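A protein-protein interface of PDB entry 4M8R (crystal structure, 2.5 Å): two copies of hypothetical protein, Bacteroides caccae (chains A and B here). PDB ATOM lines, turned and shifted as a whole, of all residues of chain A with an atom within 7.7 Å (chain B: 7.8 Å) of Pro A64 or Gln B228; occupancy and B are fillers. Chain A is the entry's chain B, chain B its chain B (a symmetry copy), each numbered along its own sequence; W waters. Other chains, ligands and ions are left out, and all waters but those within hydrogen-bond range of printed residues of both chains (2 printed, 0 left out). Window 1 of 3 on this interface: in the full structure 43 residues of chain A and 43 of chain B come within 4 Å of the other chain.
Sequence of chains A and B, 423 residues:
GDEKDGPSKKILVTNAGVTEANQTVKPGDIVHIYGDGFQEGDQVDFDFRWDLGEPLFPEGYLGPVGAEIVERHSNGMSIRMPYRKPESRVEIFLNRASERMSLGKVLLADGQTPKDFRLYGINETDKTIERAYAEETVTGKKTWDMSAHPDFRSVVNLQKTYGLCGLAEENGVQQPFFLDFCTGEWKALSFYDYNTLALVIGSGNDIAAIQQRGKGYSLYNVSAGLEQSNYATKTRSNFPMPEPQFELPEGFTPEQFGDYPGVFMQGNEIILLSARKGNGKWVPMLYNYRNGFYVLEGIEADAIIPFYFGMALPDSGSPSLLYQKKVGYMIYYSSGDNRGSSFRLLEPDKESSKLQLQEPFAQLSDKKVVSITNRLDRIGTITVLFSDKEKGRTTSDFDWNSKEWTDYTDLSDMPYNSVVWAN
Among the printed residues, merely in contact across the chains: Gly A63 with Gln B228 (3.2 Å), Phe A48 with Phe B239 (3.3 Å), Gln A228 with Pro B64 (3.5 Å), Pro A64 with Gln B228 (3.5 Å), Arg A100 with Lys B234 (3.5 Å), Pro A64 with Lys B234 (3.5 Å), Tyr A61 with Phe B239 (3.6 Å) and Gly A63 with Lys B234 (3.7 Å).
Water W1 bridges the side-chain hydroxyl (OH) of Tyr A61 (2.6 Å) and the backbone carbonyl oxygen (O) of Phe B239 (3.0 Å).
Water W2 lies within hydrogen-bond range of OD1 of Asp A47 (3.0 Å) and NZ of Lys B234 (3.3 Å).
Hydrophobic or aromatic side chains of chain B that line the printed part of chain A: Pro B64 and Phe B239.
Of the 18 printed residues of chain A, 7 touch a printed residue of chain B.
Printed residues of chain A that touch a printed residue of chain B: Asp A47, Phe A48, Tyr A61, Gly A63, Pro A64, Arg A100 and Gln A228.
Hydrophobic or aromatic side chains of chain A within 4 Å of the printed part of chain B: Tyr A61 and Pro A64.
Among the printed residues, Asp or Glu carboxylates within 4 Å of a Lys or Arg side-chain nitrogen of the other chain: Asp A47 with Lys B234 (3.1 Å).
Printed residues of chain B within 4 Å of Asp A47: Lys B234.
Printed residues of chain B within 4 Å of Phe A48: Phe B239.
Gly A63 touches two residues of chain B.
Of chain B, only Gln B228 (3.5 Å) and Lys B234 (3.5 Å) come within 4 Å of Pro A64.
Of the printed residues of chain B, Arg A100 touches Thr B233 (3.1 Å) and Lys B234 (3.5 Å).
Of the printed residues of chain B, Gln A228 touches Pro B64 (3.5 Å).
Gln B228 touches just these residues of chain A: Gly A63 and Pro A64.
Of the printed residues of chain A, Lys B234 touches Asp A47 (3.1 Å), Gly A63 (3.7 Å), Pro A64 (3.5 Å) and Arg A100 (3.5 Å).
The nearest residue of chain B that does not touch Pro A64 is Asn B230 (4.4 Å).
The nearest printed residue of chain B that does not touch Gln A228 is Asn B230 (7.0 Å).
The side-chain amide oxygen (OE1) of Gln B228 sits at hydrogen-bond distance from the backbone NH (N) of Asn B230, at 2.6 Å.
The backbone NH (N) of Tyr B231 lies close to the side-chain amide nitrogen (NE2) of Gln B228 (3.4 Å).
NE2 of Gln B228 is in hydrogen-bond range of O of Lys B234 (3.3 Å).
The side-chain hydroxyl of Thr B233 lies within hydrogen-bond range of the backbone carbonyl oxygen of Asn B230.
OD2 of Asp A45 is in salt-bridge range of NE of Arg A100, 2.9 Å away.
N of Phe A48 is in hydrogen-bond range of O of Leu A62.
The backbone carbonyl oxygen (O) of Thr B233 is in hydrogen-bond range of the guanidinium group (NH1) of Arg A100, 3.1 Å away.
NZ of Lys B234 lies within salt-bridge range of OD1 of Asp A47 (3.1 Å).
Pro A64 touches Gln B228, and with the chains exchanged Gln A228 touches Pro B64.
Of the 10 pairs that touch across the chains among the printed residues, 2 have their exchanged pair printed and touching as well.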
ATOM      1  N   VAL A  44     -17.705   2.283 -20.929  1.00  0.00           N
ATOM      2  CA  VAL A  44     -18.919   1.735 -20.351  1.00  0.00           C
ATOM      3  C   VAL A  44     -19.773   1.156 -21.467  1.00  0.00           C
ATOM      4  O   VAL A  44     -19.988   1.809 -22.483  1.00  0.00           O
ATOM      5  CB  VAL A  44     -19.701   2.814 -19.575  1.00  0.00           C
ATOM      6  CG1 VAL A  44     -21.019   2.259 -19.049  1.00  0.00           C
ATOM      7  CG2 VAL A  44     -18.859   3.357 -18.432  1.00  0.00           C
ATOM      8  N   ASP A  45     -20.248  -0.073 -21.257  1.00  0.00           N
ATOM      9  CA  ASP A  45     -21.053  -0.812 -22.232  1.00  0.00           C
ATOM     10  C   ASP A  45     -22.453  -1.064 -21.692  1.00  0.00           C
ATOM     11  O   ASP A  45     -22.639  -1.278 -20.498  1.00  0.00           O
ATOM     12  CB  ASP A  45     -20.418  -2.174 -22.534  1.00  0.00           C
ATOM     13  CG  ASP A  45     -19.248  -2.086 -23.482  1.00  0.00           C
ATOM     14  OD1 ASP A  45     -19.309  -1.306 -24.460  1.00  0.00           O
ATOM     15  OD2 ASP A  45     -18.266  -2.825 -23.263  1.00  0.00           O
ATOM     16  N   PHE A  46     -23.423  -1.066 -22.598  1.00  0.00           N
ATOM     17  CA  PHE A  46     -24.796  -1.428 -22.297  1.00  0.00           C
ATOM     18  C   PHE A  46     -25.118  -2.778 -22.929  1.00  0.00           C
ATOM     19  O   PHE A  46     -24.668  -3.065 -24.037  1.00  0.00           O
ATOM     20  CB  PHE A  46     -25.766  -0.429 -22.921  1.00  0.00           C
ATOM     21  CG  PHE A  46     -25.716   0.946 -22.336  1.00  0.00           C
ATOM     22  CD1 PHE A  46     -25.777   1.149 -20.967  1.00  0.00           C
ATOM     23  CD2 PHE A  46     -25.683   2.052 -23.171  1.00  0.00           C
ATOM     24  CE1 PHE A  46     -25.764   2.429 -20.438  1.00  0.00           C
ATOM     25  CE2 PHE A  46     -25.671   3.333 -22.651  1.00  0.00           C
ATOM     26  CZ  PHE A  46     -25.716   3.520 -21.281  1.00  0.00           C
ATOM     27  N   ASP A  47     -25.918  -3.582 -22.233  1.00  0.00           N
ATOM     28  CA  ASP A  47     -26.611  -4.721 -22.843  1.00  0.00           C
ATOM     29  C   ASP A  47     -28.108  -4.499 -22.644  1.00  0.00           C
ATOM     30  O   ASP A  47     -28.552  -4.223 -21.534  1.00  0.00           O
ATOM     31  CB  ASP A  47     -26.184  -6.058 -22.215  1.00  0.00           C
ATOM     32  CG  ASP A  47     -24.847  -6.587 -22.768  1.00  0.00           C
ATOM     33  OD1 ASP A  47     -24.183  -5.901 -23.584  1.00  0.00           O
ATOM     34  OD2 ASP A  47     -24.447  -7.709 -22.376  1.00  0.00           O
ATOM     35  N   PHE A  48     -28.874  -4.610 -23.727  1.00  0.00           N
ATOM     36  CA  PHE A  48     -30.309  -4.364 -23.705  1.00  0.00           C
ATOM     37  C   PHE A  48     -31.073  -5.676 -23.835  1.00  0.00           C
ATOM     38  O   PHE A  48     -30.687  -6.553 -24.609  1.00  0.00           O
ATOM     39  CB  PHE A  48     -30.711  -3.449 -24.865  1.00  0.00           C
ATOM     40  CG  PHE A  48     -30.090  -2.080 -24.814  1.00  0.00           C
ATOM     41  CD1 PHE A  48     -28.783  -1.882 -25.222  1.00  0.00           C
ATOM     42  CD2 PHE A  48     -30.824  -0.986 -24.377  1.00  0.00           C
ATOM     43  CE1 PHE A  48     -28.211  -0.619 -25.180  1.00  0.00           C
ATOM     44  CE2 PHE A  48     -30.261   0.271 -24.318  1.00  0.00           C
ATOM     45  CZ  PHE A  48     -28.948   0.457 -24.720  1.00  0.00           C
ATOM     46  N   TYR A  61     -32.554  -8.604 -28.066  1.00  0.00           N
ATOM     47  CA  TYR A  61     -31.268  -8.426 -27.397  1.00  0.00           C
ATOM     48  C   TYR A  61     -30.399  -7.475 -28.172  1.00  0.00           C
ATOM     49  O   TYR A  61     -30.456  -7.429 -29.386  1.00  0.00           O
ATOM     50  CB  TYR A  61     -30.521  -9.755 -27.264  1.00  0.00           C
ATOM     51  CG  TYR A  61     -31.367 -10.874 -26.737  1.00  0.00           C
ATOM     52  CD1 TYR A  61     -31.703 -10.940 -25.386  1.00  0.00           C
ATOM     53  CD2 TYR A  61     -31.828 -11.872 -27.580  1.00  0.00           C
ATOM     54  CE1 TYR A  61     -32.483 -11.971 -24.894  1.00  0.00           C
ATOM     55  CE2 TYR A  61     -32.610 -12.905 -27.096  1.00  0.00           C
ATOM     56  CZ  TYR A  61     -32.933 -12.948 -25.754  1.00  0.00           C
ATOM     57  OH  TYR A  61     -33.717 -13.968 -25.272  1.00  0.00           O
ATOM     58  N   LEU A  62     -29.575  -6.733 -27.454  1.00  0.00           N
ATOM     59  CA  LEU A  62     -28.580  -5.884 -28.074  1.00  0.00           C
ATOM     60  C   LEU A  62     -27.439  -5.686 -27.095  1.00  0.00           C
ATOM     61  O   LEU A  62     -27.670  -5.524 -25.901  1.00  0.00           O
ATOM     62  CB  LEU A  62     -29.199  -4.549 -28.455  1.00  0.00           C
ATOM     63  CG  LEU A  62     -28.349  -3.641 -29.336  1.00  0.00           C
ATOM     64  CD1 LEU A  62     -28.041  -4.302 -30.674  1.00  0.00           C
ATOM     65  CD2 LEU A  62     -29.067  -2.312 -29.531  1.00  0.00           C
ATOM     66  N   GLY A  63     -26.209  -5.730 -27.592  1.00  0.00           N
ATOM     67  CA  GLY A  63     -25.039  -5.576 -26.735  1.00  0.00           C
ATOM     68  C   GLY A  63     -23.790  -6.221 -27.308  1.00  0.00           C
ATOM     69  O   GLY A  63     -23.880  -7.245 -27.983  1.00  0.00           O
ATOM     70  N   PRO A  64     -22.611  -5.632 -27.039  1.00  0.00           N
ATOM     71  CA  PRO A  64     -22.371  -4.431 -26.247  1.00  0.00           C
ATOM     72  C   PRO A  64     -22.565  -3.156 -27.066  1.00  0.00           C
ATOM     73  O   PRO A  64     -22.179  -3.098 -28.232  1.00  0.00           O
ATOM     74  CB  PRO A  64     -20.907  -4.577 -25.861  1.00  0.00           C
ATOM     75  CG  PRO A  64     -20.292  -5.256 -27.044  1.00  0.00           C
ATOM     76  CD  PRO A  64     -21.368  -6.101 -27.682  1.00  0.00           C
ATOM     77  N   VAL A  65     -23.171  -2.154 -26.452  1.00  0.00           N
ATOM     78  CA  VAL A  65     -23.365  -0.868 -27.078  1.00  0.00           C
ATOM     79  C   VAL A  65     -22.657   0.121 -26.175  1.00  0.00           C
ATOM     80  O   VAL A  65     -22.991   0.233 -24.998  1.00  0.00           O
ATOM     81  CB  VAL A  65     -24.860  -0.519 -27.185  1.00  0.00           C
ATOM     82  CG1 VAL A  65     -25.071   0.844 -27.835  1.00  0.00           C
ATOM     83  CG2 VAL A  65     -25.595  -1.600 -27.962  1.00  0.00           C
ATOM     84  N   GLY A  66     -21.651   0.804 -26.717  1.00  0.00           N
ATOM     85  CA  GLY A  66     -20.876   1.761 -25.956  1.00  0.00           C
ATOM     86  C   GLY A  66     -21.757   2.879 -25.457  1.00  0.00           C
ATOM     87  O   GLY A  66     -22.624   3.358 -26.180  1.00  0.00           O
ATOM     88  N   ALA A  67     -21.556   3.269 -24.203  1.00  0.00           N
ATOM     89  CA  ALA A  67     -22.286   4.378 -23.611  1.00  0.00           C
ATOM     90  C   ALA A  67     -21.505   5.658 -23.815  1.00  0.00           C
ATOM     91  O   ALA A  67     -20.279   5.659 -23.710  1.00  0.00           O
ATOM     92  CB  ALA A  67     -22.493   4.132 -22.125  1.00  0.00           C
ATOM     93  N   PHE A  93     -22.089  -2.097 -17.844  1.00  0.00           N
ATOM     94  CA  PHE A  93     -20.795  -2.740 -17.594  1.00  0.00           C
ATOM     95  C   PHE A  93     -19.632  -1.756 -17.674  1.00  0.00           C
ATOM     96  O   PHE A  93     -19.576  -0.927 -18.575  1.00  0.00           O
ATOM     97  CB  PHE A  93     -20.533  -3.835 -18.633  1.00  0.00           C
ATOM     98  CG  PHE A  93     -21.515  -4.960 -18.595  1.00  0.00           C
ATOM     99  CD1 PHE A  93     -21.304  -6.056 -17.769  1.00  0.00           C
ATOM    100  CD2 PHE A  93     -22.652  -4.932 -19.387  1.00  0.00           C
ATOM    101  CE1 PHE A  93     -22.214  -7.094 -17.726  1.00  0.00           C
ATOM    102  CE2 PHE A  93     -23.564  -5.973 -19.350  1.00  0.00           C
ATOM    103  CZ  PHE A  93     -23.345  -7.053 -18.520  1.00  0.00           C
ATOM    104  N   ASN A  95     -15.931  -1.363 -18.766  1.00  0.00           N
ATOM    105  CA  ASN A  95     -15.075  -2.042 -19.735  1.00  0.00           C
ATOM    106  C   ASN A  95     -13.653  -1.491 -19.673  1.00  0.00           C
ATOM    107  O   ASN A  95     -13.402  -0.368 -20.113  1.00  0.00           O
ATOM    108  CB  ASN A  95     -15.661  -1.870 -21.141  1.00  0.00           C
ATOM    109  CG  ASN A  95     -14.872  -2.608 -22.214  1.00  0.00           C
ATOM    110  OD1 ASN A  95     -13.958  -3.381 -21.924  1.00  0.00           O
ATOM    111  ND2 ASN A  95     -15.238  -2.380 -23.467  1.00  0.00           N
ATOM    112  N   ARG A 100     -14.656  -6.994 -18.427  1.00  0.00           N
ATOM    113  CA  ARG A 100     -15.939  -6.351 -18.128  1.00  0.00           C
ATOM    114  C   ARG A 100     -16.387  -6.656 -16.691  1.00  0.00           C
ATOM    115  O   ARG A 100     -16.143  -7.745 -16.179  1.00  0.00           O
ATOM    116  CB  ARG A 100     -17.011  -6.788 -19.121  1.00  0.00           C
ATOM    117  CG  ARG A 100     -16.889  -6.085 -20.462  1.00  0.00           C
ATOM    118  CD  ARG A 100     -18.050  -6.378 -21.396  1.00  0.00           C
ATOM    119  NE  ARG A 100     -17.933  -5.596 -22.634  1.00  0.00           N
ATOM    120  CZ  ARG A 100     -17.149  -5.901 -23.677  1.00  0.00           C
ATOM    121  NH1 ARG A 100     -16.379  -6.986 -23.669  1.00  0.00           N
ATOM    122  NH2 ARG A 100     -17.134  -5.108 -24.742  1.00  0.00           N
ATOM    123  N   GLN A 228     -25.788   1.640 -37.838  1.00  0.00           N
ATOM    124  CA  GLN A 228     -24.841   0.771 -37.155  1.00  0.00           C
ATOM    125  C   GLN A 228     -24.984   0.956 -35.635  1.00  0.00           C
ATOM    126  O   GLN A 228     -25.044   2.086 -35.147  1.00  0.00           O
ATOM    127  CB  GLN A 228     -23.448   1.108 -37.699  1.00  0.00           C
ATOM    128  CG  GLN A 228     -22.260   0.657 -36.896  1.00  0.00           C
ATOM    129  CD  GLN A 228     -21.938   1.566 -35.717  1.00  0.00           C
ATOM    130  OE1 GLN A 228     -21.751   1.074 -34.620  1.00  0.00           O
ATOM    131  NE2 GLN A 228     -21.868   2.879 -35.937  1.00  0.00           N
ATOM    132  N   SER A 229     -25.052  -0.157 -34.901  1.00  0.00           N
ATOM    133  CA  SER A 229     -25.572  -0.160 -33.514  1.00  0.00           C
ATOM    134  C   SER A 229     -24.771   0.621 -32.460  1.00  0.00           C
ATOM    135  O   SER A 229     -25.304   0.928 -31.380  1.00  0.00           O
ATOM    136  CB  SER A 229     -25.792  -1.599 -33.032  1.00  0.00           C
ATOM    137  OG  SER A 229     -24.582  -2.333 -33.000  1.00  0.00           O
ATOM    138  N   ASN A 230     -23.514   0.939 -32.766  1.00  0.00           N
ATOM    139  CA  ASN A 230     -22.699   1.832 -31.933  1.00  0.00           C
ATOM    140  C   ASN A 230     -22.623   3.280 -32.452  1.00  0.00           C
ATOM    141  O   ASN A 230     -21.635   3.984 -32.207  1.00  0.00           O
ATOM    142  CB  ASN A 230     -21.291   1.250 -31.739  1.00  0.00           C
ATOM    143  CG  ASN A 230     -21.209   0.334 -30.546  1.00  0.00           C
ATOM    144  OD1 ASN A 230     -21.460   0.754 -29.422  1.00  0.00           O
ATOM    145  ND2 ASN A 230     -20.832  -0.913 -30.775  1.00  0.00           N
ATOM    146  N   PRO B  64     -17.541   0.027 -35.983  1.00  0.00           N
ATOM    147  CA  PRO B  64     -16.265  -0.441 -35.452  1.00  0.00           C
ATOM    148  C   PRO B  64     -16.364  -1.857 -34.889  1.00  0.00           C
ATOM    149  O   PRO B  64     -17.354  -2.208 -34.251  1.00  0.00           O
ATOM    150  CB  PRO B  64     -15.996   0.543 -34.325  1.00  0.00           C
ATOM    151  CG  PRO B  64     -17.358   0.860 -33.795  1.00  0.00           C
ATOM    152  CD  PRO B  64     -18.328   0.716 -34.943  1.00  0.00           C
ATOM    153  N   VAL B  65     -15.342  -2.660 -35.140  1.00  0.00           N
ATOM    154  CA  VAL B  65     -15.267  -4.001 -34.617  1.00  0.00           C
ATOM    155  C   VAL B  65     -13.996  -4.033 -33.792  1.00  0.00           C
ATOM    156  O   VAL B  65     -12.913  -3.783 -34.316  1.00  0.00           O
ATOM    157  CB  VAL B  65     -15.194  -5.039 -35.752  1.00  0.00           C
ATOM    158  CG1 VAL B  65     -15.102  -6.459 -35.206  1.00  0.00           C
ATOM    159  CG2 VAL B  65     -16.399  -4.897 -36.669  1.00  0.00           C
ATOM    160  N   LYS B  85     -14.961 -12.587 -41.936  1.00  0.00           N
ATOM    161  CA  LYS B  85     -15.282 -11.512 -42.868  1.00  0.00           C
ATOM    162  C   LYS B  85     -14.813 -11.909 -44.259  1.00  0.00           C
ATOM    163  O   LYS B  85     -13.924 -12.747 -44.397  1.00  0.00           O
ATOM    164  CB  LYS B  85     -14.607 -10.208 -42.458  1.00  0.00           C
ATOM    165  CG  LYS B  85     -14.634  -9.900 -40.974  1.00  0.00           C
ATOM    166  CD  LYS B  85     -16.043  -9.776 -40.423  1.00  0.00           C
ATOM    167  CE  LYS B  85     -16.007  -9.519 -38.922  1.00  0.00           C
ATOM    168  NZ  LYS B  85     -15.220 -10.538 -38.170  1.00  0.00           N
ATOM    169  N   SER B 223     -26.413 -17.660 -26.502  1.00  0.00           N
ATOM    170  CA  SER B 223     -25.766 -17.571 -27.809  1.00  0.00           C
ATOM    171  C   SER B 223     -25.764 -16.147 -28.375  1.00  0.00           C
ATOM    172  O   SER B 223     -25.102 -15.893 -29.385  1.00  0.00           O
ATOM    173  CB  SER B 223     -26.430 -18.521 -28.801  1.00  0.00           C
ATOM    174  OG  SER B 223     -27.775 -18.155 -29.032  1.00  0.00           O
ATOM    175  N   ALA B 224     -26.475 -15.223 -27.726  1.00  0.00           N
ATOM    176  CA  ALA B 224     -26.554 -13.838 -28.199  1.00  0.00           C
ATOM    177  C   ALA B 224     -25.187 -13.193 -28.453  1.00  0.00           C
ATOM    178  O   ALA B 224     -25.061 -12.374 -29.356  1.00  0.00           O
ATOM    179  CB  ALA B 224     -27.364 -12.986 -27.230  1.00  0.00           C
ATOM    180  N   GLY B 225     -24.184 -13.551 -27.649  1.00  0.00           N
ATOM    181  CA  GLY B 225     -22.816 -13.049 -27.825  1.00  0.00           C
ATOM    182  C   GLY B 225     -22.138 -13.537 -29.095  1.00  0.00           C
ATOM    183  O   GLY B 225     -21.226 -12.894 -29.601  1.00  0.00           O
ATOM    184  N   LEU B 226     -22.580 -14.672 -29.618  1.00  0.00           N
ATOM    185  CA  LEU B 226     -22.053 -15.183 -30.878  1.00  0.00           C
ATOM    186  C   LEU B 226     -22.720 -14.546 -32.091  1.00  0.00           C
ATOM    187  O   LEU B 226     -22.089 -14.381 -33.131  1.00  0.00           O
ATOM    188  CB  LEU B 226     -22.243 -16.696 -30.954  1.00  0.00           C
ATOM    189  CG  LEU B 226     -21.566 -17.531 -29.869  1.00  0.00           C
ATOM    190  CD1 LEU B 226     -21.952 -18.989 -30.045  1.00  0.00           C
ATOM    191  CD2 LEU B 226     -20.053 -17.375 -29.900  1.00  0.00           C
ATOM    192  N   GLU B 227     -23.994 -14.198 -31.970  1.00  0.00           N
ATOM    193  CA  GLU B 227     -24.768 -13.695 -33.110  1.00  0.00           C
ATOM    194  C   GLU B 227     -24.679 -12.175 -33.224  1.00  0.00           C
ATOM    195  O   GLU B 227     -25.681 -11.490 -33.437  1.00  0.00           O
ATOM    196  CB  GLU B 227     -26.233 -14.147 -32.993  1.00  0.00           C
ATOM    197  CG  GLU B 227     -26.435 -15.624 -33.293  1.00  0.00           C
ATOM    198  CD  GLU B 227     -26.269 -15.943 -34.770  1.00  0.00           C
ATOM    199  OE1 GLU B 227     -27.217 -15.674 -35.538  1.00  0.00           O
ATOM    200  OE2 GLU B 227     -25.198 -16.456 -35.166  1.00  0.00           O
ATOM    201  N   GLN B 228     -23.467 -11.650 -33.130  1.00  0.00           N
ATOM    202  CA  GLN B 228     -23.288 -10.236 -32.831  1.00  0.00           C
ATOM    203  C   GLN B 228     -21.870  -9.805 -33.238  1.00  0.00           C
ATOM    204  O   GLN B 228     -20.895 -10.492 -32.928  1.00  0.00           O
ATOM    205  CB  GLN B 228     -23.599 -10.050 -31.342  1.00  0.00           C
ATOM    206  CG  GLN B 228     -23.112  -8.789 -30.684  1.00  0.00           C
ATOM    207  CD  GLN B 228     -21.640  -8.830 -30.297  1.00  0.00           C
ATOM    208  OE1 GLN B 228     -20.919  -7.898 -30.601  1.00  0.00           O
ATOM    209  NE2 GLN B 228     -21.195  -9.894 -29.627  1.00  0.00           N
ATOM    210  N   SER B 229     -21.766  -8.675 -33.942  1.00  0.00           N
ATOM    211  CA  SER B 229     -20.556  -8.338 -34.726  1.00  0.00           C
ATOM    212  C   SER B 229     -19.254  -8.102 -33.944  1.00  0.00           C
ATOM    213  O   SER B 229     -18.163  -8.137 -34.536  1.00  0.00           O
ATOM    214  CB  SER B 229     -20.833  -7.139 -35.642  1.00  0.00           C
ATOM    215  OG  SER B 229     -21.158  -5.977 -34.901  1.00  0.00           O
ATOM    216  N   ASN B 230     -19.366  -7.864 -32.638  1.00  0.00           N
ATOM    217  CA  ASN B 230     -18.202  -7.801 -31.744  1.00  0.00           C
ATOM    218  C   ASN B 230     -17.954  -9.092 -30.942  1.00  0.00           C
ATOM    219  O   ASN B 230     -17.397  -9.047 -29.837  1.00  0.00           O
ATOM    220  CB  ASN B 230     -18.312  -6.590 -30.805  1.00  0.00           C
ATOM    221  CG  ASN B 230     -17.713  -5.345 -31.402  1.00  0.00           C
ATOM    222  OD1 ASN B 230     -16.527  -5.312 -31.710  1.00  0.00           O
ATOM    223  ND2 ASN B 230     -18.517  -4.304 -31.546  1.00  0.00           N
ATOM    224  N   TYR B 231     -18.385 -10.225 -31.506  1.00  0.00           N
ATOM    225  CA  TYR B 231     -18.138 -11.528 -30.905  1.00  0.00           C
ATOM    226  C   TYR B 231     -16.670 -11.717 -30.480  1.00  0.00           C
ATOM    227  O   TYR B 231     -16.417 -12.241 -29.403  1.00  0.00           O
ATOM    228  CB  TYR B 231     -18.638 -12.630 -31.835  1.00  0.00           C
ATOM    229  CG  TYR B 231     -17.940 -12.680 -33.173  1.00  0.00           C
ATOM    230  CD1 TYR B 231     -16.786 -13.417 -33.332  1.00  0.00           C
ATOM    231  CD2 TYR B 231     -18.434 -11.983 -34.271  1.00  0.00           C
ATOM    232  CE1 TYR B 231     -16.140 -13.460 -34.542  1.00  0.00           C
ATOM    233  CE2 TYR B 231     -17.793 -12.027 -35.490  1.00  0.00           C
ATOM    234  CZ  TYR B 231     -16.644 -12.767 -35.616  1.00  0.00           C
ATOM    235  OH  TYR B 231     -15.995 -12.816 -36.816  1.00  0.00           O
ATOM    236  N   ALA B 232     -15.723 -11.263 -31.302  1.00  0.00           N
ATOM    237  CA  ALA B 232     -14.295 -11.476 -31.033  1.00  0.00           C
ATOM    238  C   ALA B 232     -13.851 -10.990 -29.644  1.00  0.00           C
ATOM    239  O   ALA B 232     -13.023 -11.629 -28.995  1.00  0.00           O
ATOM    240  CB  ALA B 232     -13.454 -10.815 -32.117  1.00  0.00           C
ATOM    241  N   THR B 233     -14.412  -9.869 -29.196  1.00  0.00           N
ATOM    242  CA  THR B 233     -14.033  -9.244 -27.926  1.00  0.00           C
ATOM    243  C   THR B 233     -15.099  -9.349 -26.832  1.00  0.00           C
ATOM    244  O   THR B 233     -14.895  -8.848 -25.729  1.00  0.00           O
ATOM    245  CB  THR B 233     -13.701  -7.747 -28.138  1.00  0.00           C
ATOM    246  OG1 THR B 233     -14.792  -7.077 -28.796  1.00  0.00           O
ATOM    247  CG2 THR B 233     -12.443  -7.604 -28.979  1.00  0.00           C
ATOM    248  N   LYS B 234     -16.225  -9.988 -27.134  1.00  0.00           N
ATOM    249  CA  LYS B 234     -17.353 -10.047 -26.199  1.00  0.00           C
ATOM    250  C   LYS B 234     -18.283 -11.218 -26.545  1.00  0.00           C
ATOM    251  O   LYS B 234     -18.973 -11.194 -27.568  1.00  0.00           O
ATOM    252  CB  LYS B 234     -18.098  -8.699 -26.193  1.00  0.00           C
ATOM    253  CG  LYS B 234     -19.590  -8.720 -25.840  1.00  0.00           C
ATOM    254  CD  LYS B 234     -19.899  -9.153 -24.417  1.00  0.00           C
ATOM    255  CE  LYS B 234     -21.402  -9.323 -24.195  1.00  0.00           C
ATOM    256  NZ  LYS B 234     -22.232  -8.144 -24.575  1.00  0.00           N
ATOM    257  N   THR B 235     -18.273 -12.239 -25.693  1.00  0.00           N
ATOM    258  CA  THR B 235     -19.064 -13.452 -25.904  1.00  0.00           C
ATOM    259  C   THR B 235     -19.974 -13.823 -24.735  1.00  0.00           C
ATOM    260  O   THR B 235     -20.987 -14.480 -24.943  1.00  0.00           O
ATOM    261  CB  THR B 235     -18.160 -14.669 -26.187  1.00  0.00           C
ATOM    262  OG1 THR B 235     -17.361 -14.969 -25.034  1.00  0.00           O
ATOM    263  CG2 THR B 235     -17.258 -14.397 -27.363  1.00  0.00           C
ATOM    264  N   ARG B 236     -19.604 -13.438 -23.516  1.00  0.00           N
ATOM    265  CA  ARG B 236     -20.393 -13.768 -22.339  1.00  0.00           C
ATOM    266  C   ARG B 236     -21.672 -12.943 -22.319  1.00  0.00           C
ATOM    267  O   ARG B 236     -21.619 -11.733 -22.447  1.00  0.00           O
ATOM    268  CB  ARG B 236     -19.604 -13.492 -21.068  1.00  0.00           C
ATOM    269  CG  ARG B 236     -18.341 -14.315 -20.897  1.00  0.00           C
ATOM    270  CD  ARG B 236     -17.585 -13.897 -19.641  1.00  0.00           C
ATOM    271  NE  ARG B 236     -16.193 -14.351 -19.681  1.00  0.00           N
ATOM    272  CZ  ARG B 236     -15.645 -15.285 -18.897  1.00  0.00           C
ATOM    273  NH1 ARG B 236     -16.345 -15.900 -17.947  1.00  0.00           N
ATOM    274  NH2 ARG B 236     -14.363 -15.599 -19.066  1.00  0.00           N
ATOM    275  N   SER B 237     -22.813 -13.600 -22.149  1.00  0.00           N
ATOM    276  CA  SER B 237     -24.108 -12.931 -22.086  1.00  0.00           C
ATOM    277  C   SER B 237     -24.699 -13.081 -20.699  1.00  0.00           C
ATOM    278  O   SER B 237     -24.342 -14.000 -19.965  1.00  0.00           O
ATOM    279  CB  SER B 237     -25.091 -13.560 -23.074  1.00  0.00           C
ATOM    280  OG  SER B 237     -24.619 -13.502 -24.408  1.00  0.00           O
ATOM    281  N   PHE B 239     -28.606 -12.810 -20.123  1.00  0.00           N
ATOM    282  CA  PHE B 239     -29.946 -12.509 -20.617  1.00  0.00           C
ATOM    283  C   PHE B 239     -30.994 -13.494 -20.109  1.00  0.00           C
ATOM    284  O   PHE B 239     -31.488 -14.325 -20.867  1.00  0.00           O
ATOM    285  CB  PHE B 239     -29.950 -12.514 -22.153  1.00  0.00           C
ATOM    286  CG  PHE B 239     -29.267 -11.334 -22.781  1.00  0.00           C
ATOM    287  CD1 PHE B 239     -29.619 -10.042 -22.431  1.00  0.00           C
ATOM    288  CD2 PHE B 239     -28.311 -11.518 -23.768  1.00  0.00           C
ATOM    289  CE1 PHE B 239     -29.010  -8.955 -23.027  1.00  0.00           C
ATOM    290  CE2 PHE B 239     -27.692 -10.436 -24.367  1.00  0.00           C
ATOM    291  CZ  PHE B 239     -28.045  -9.152 -23.996  1.00  0.00           C
HETATM  292  O   HOH W   1     -33.837 -14.532 -22.711  1.00  0.00           O
HETATM  293  O   HOH W   2     -21.456  -5.786 -22.437  1.00  0.00           O
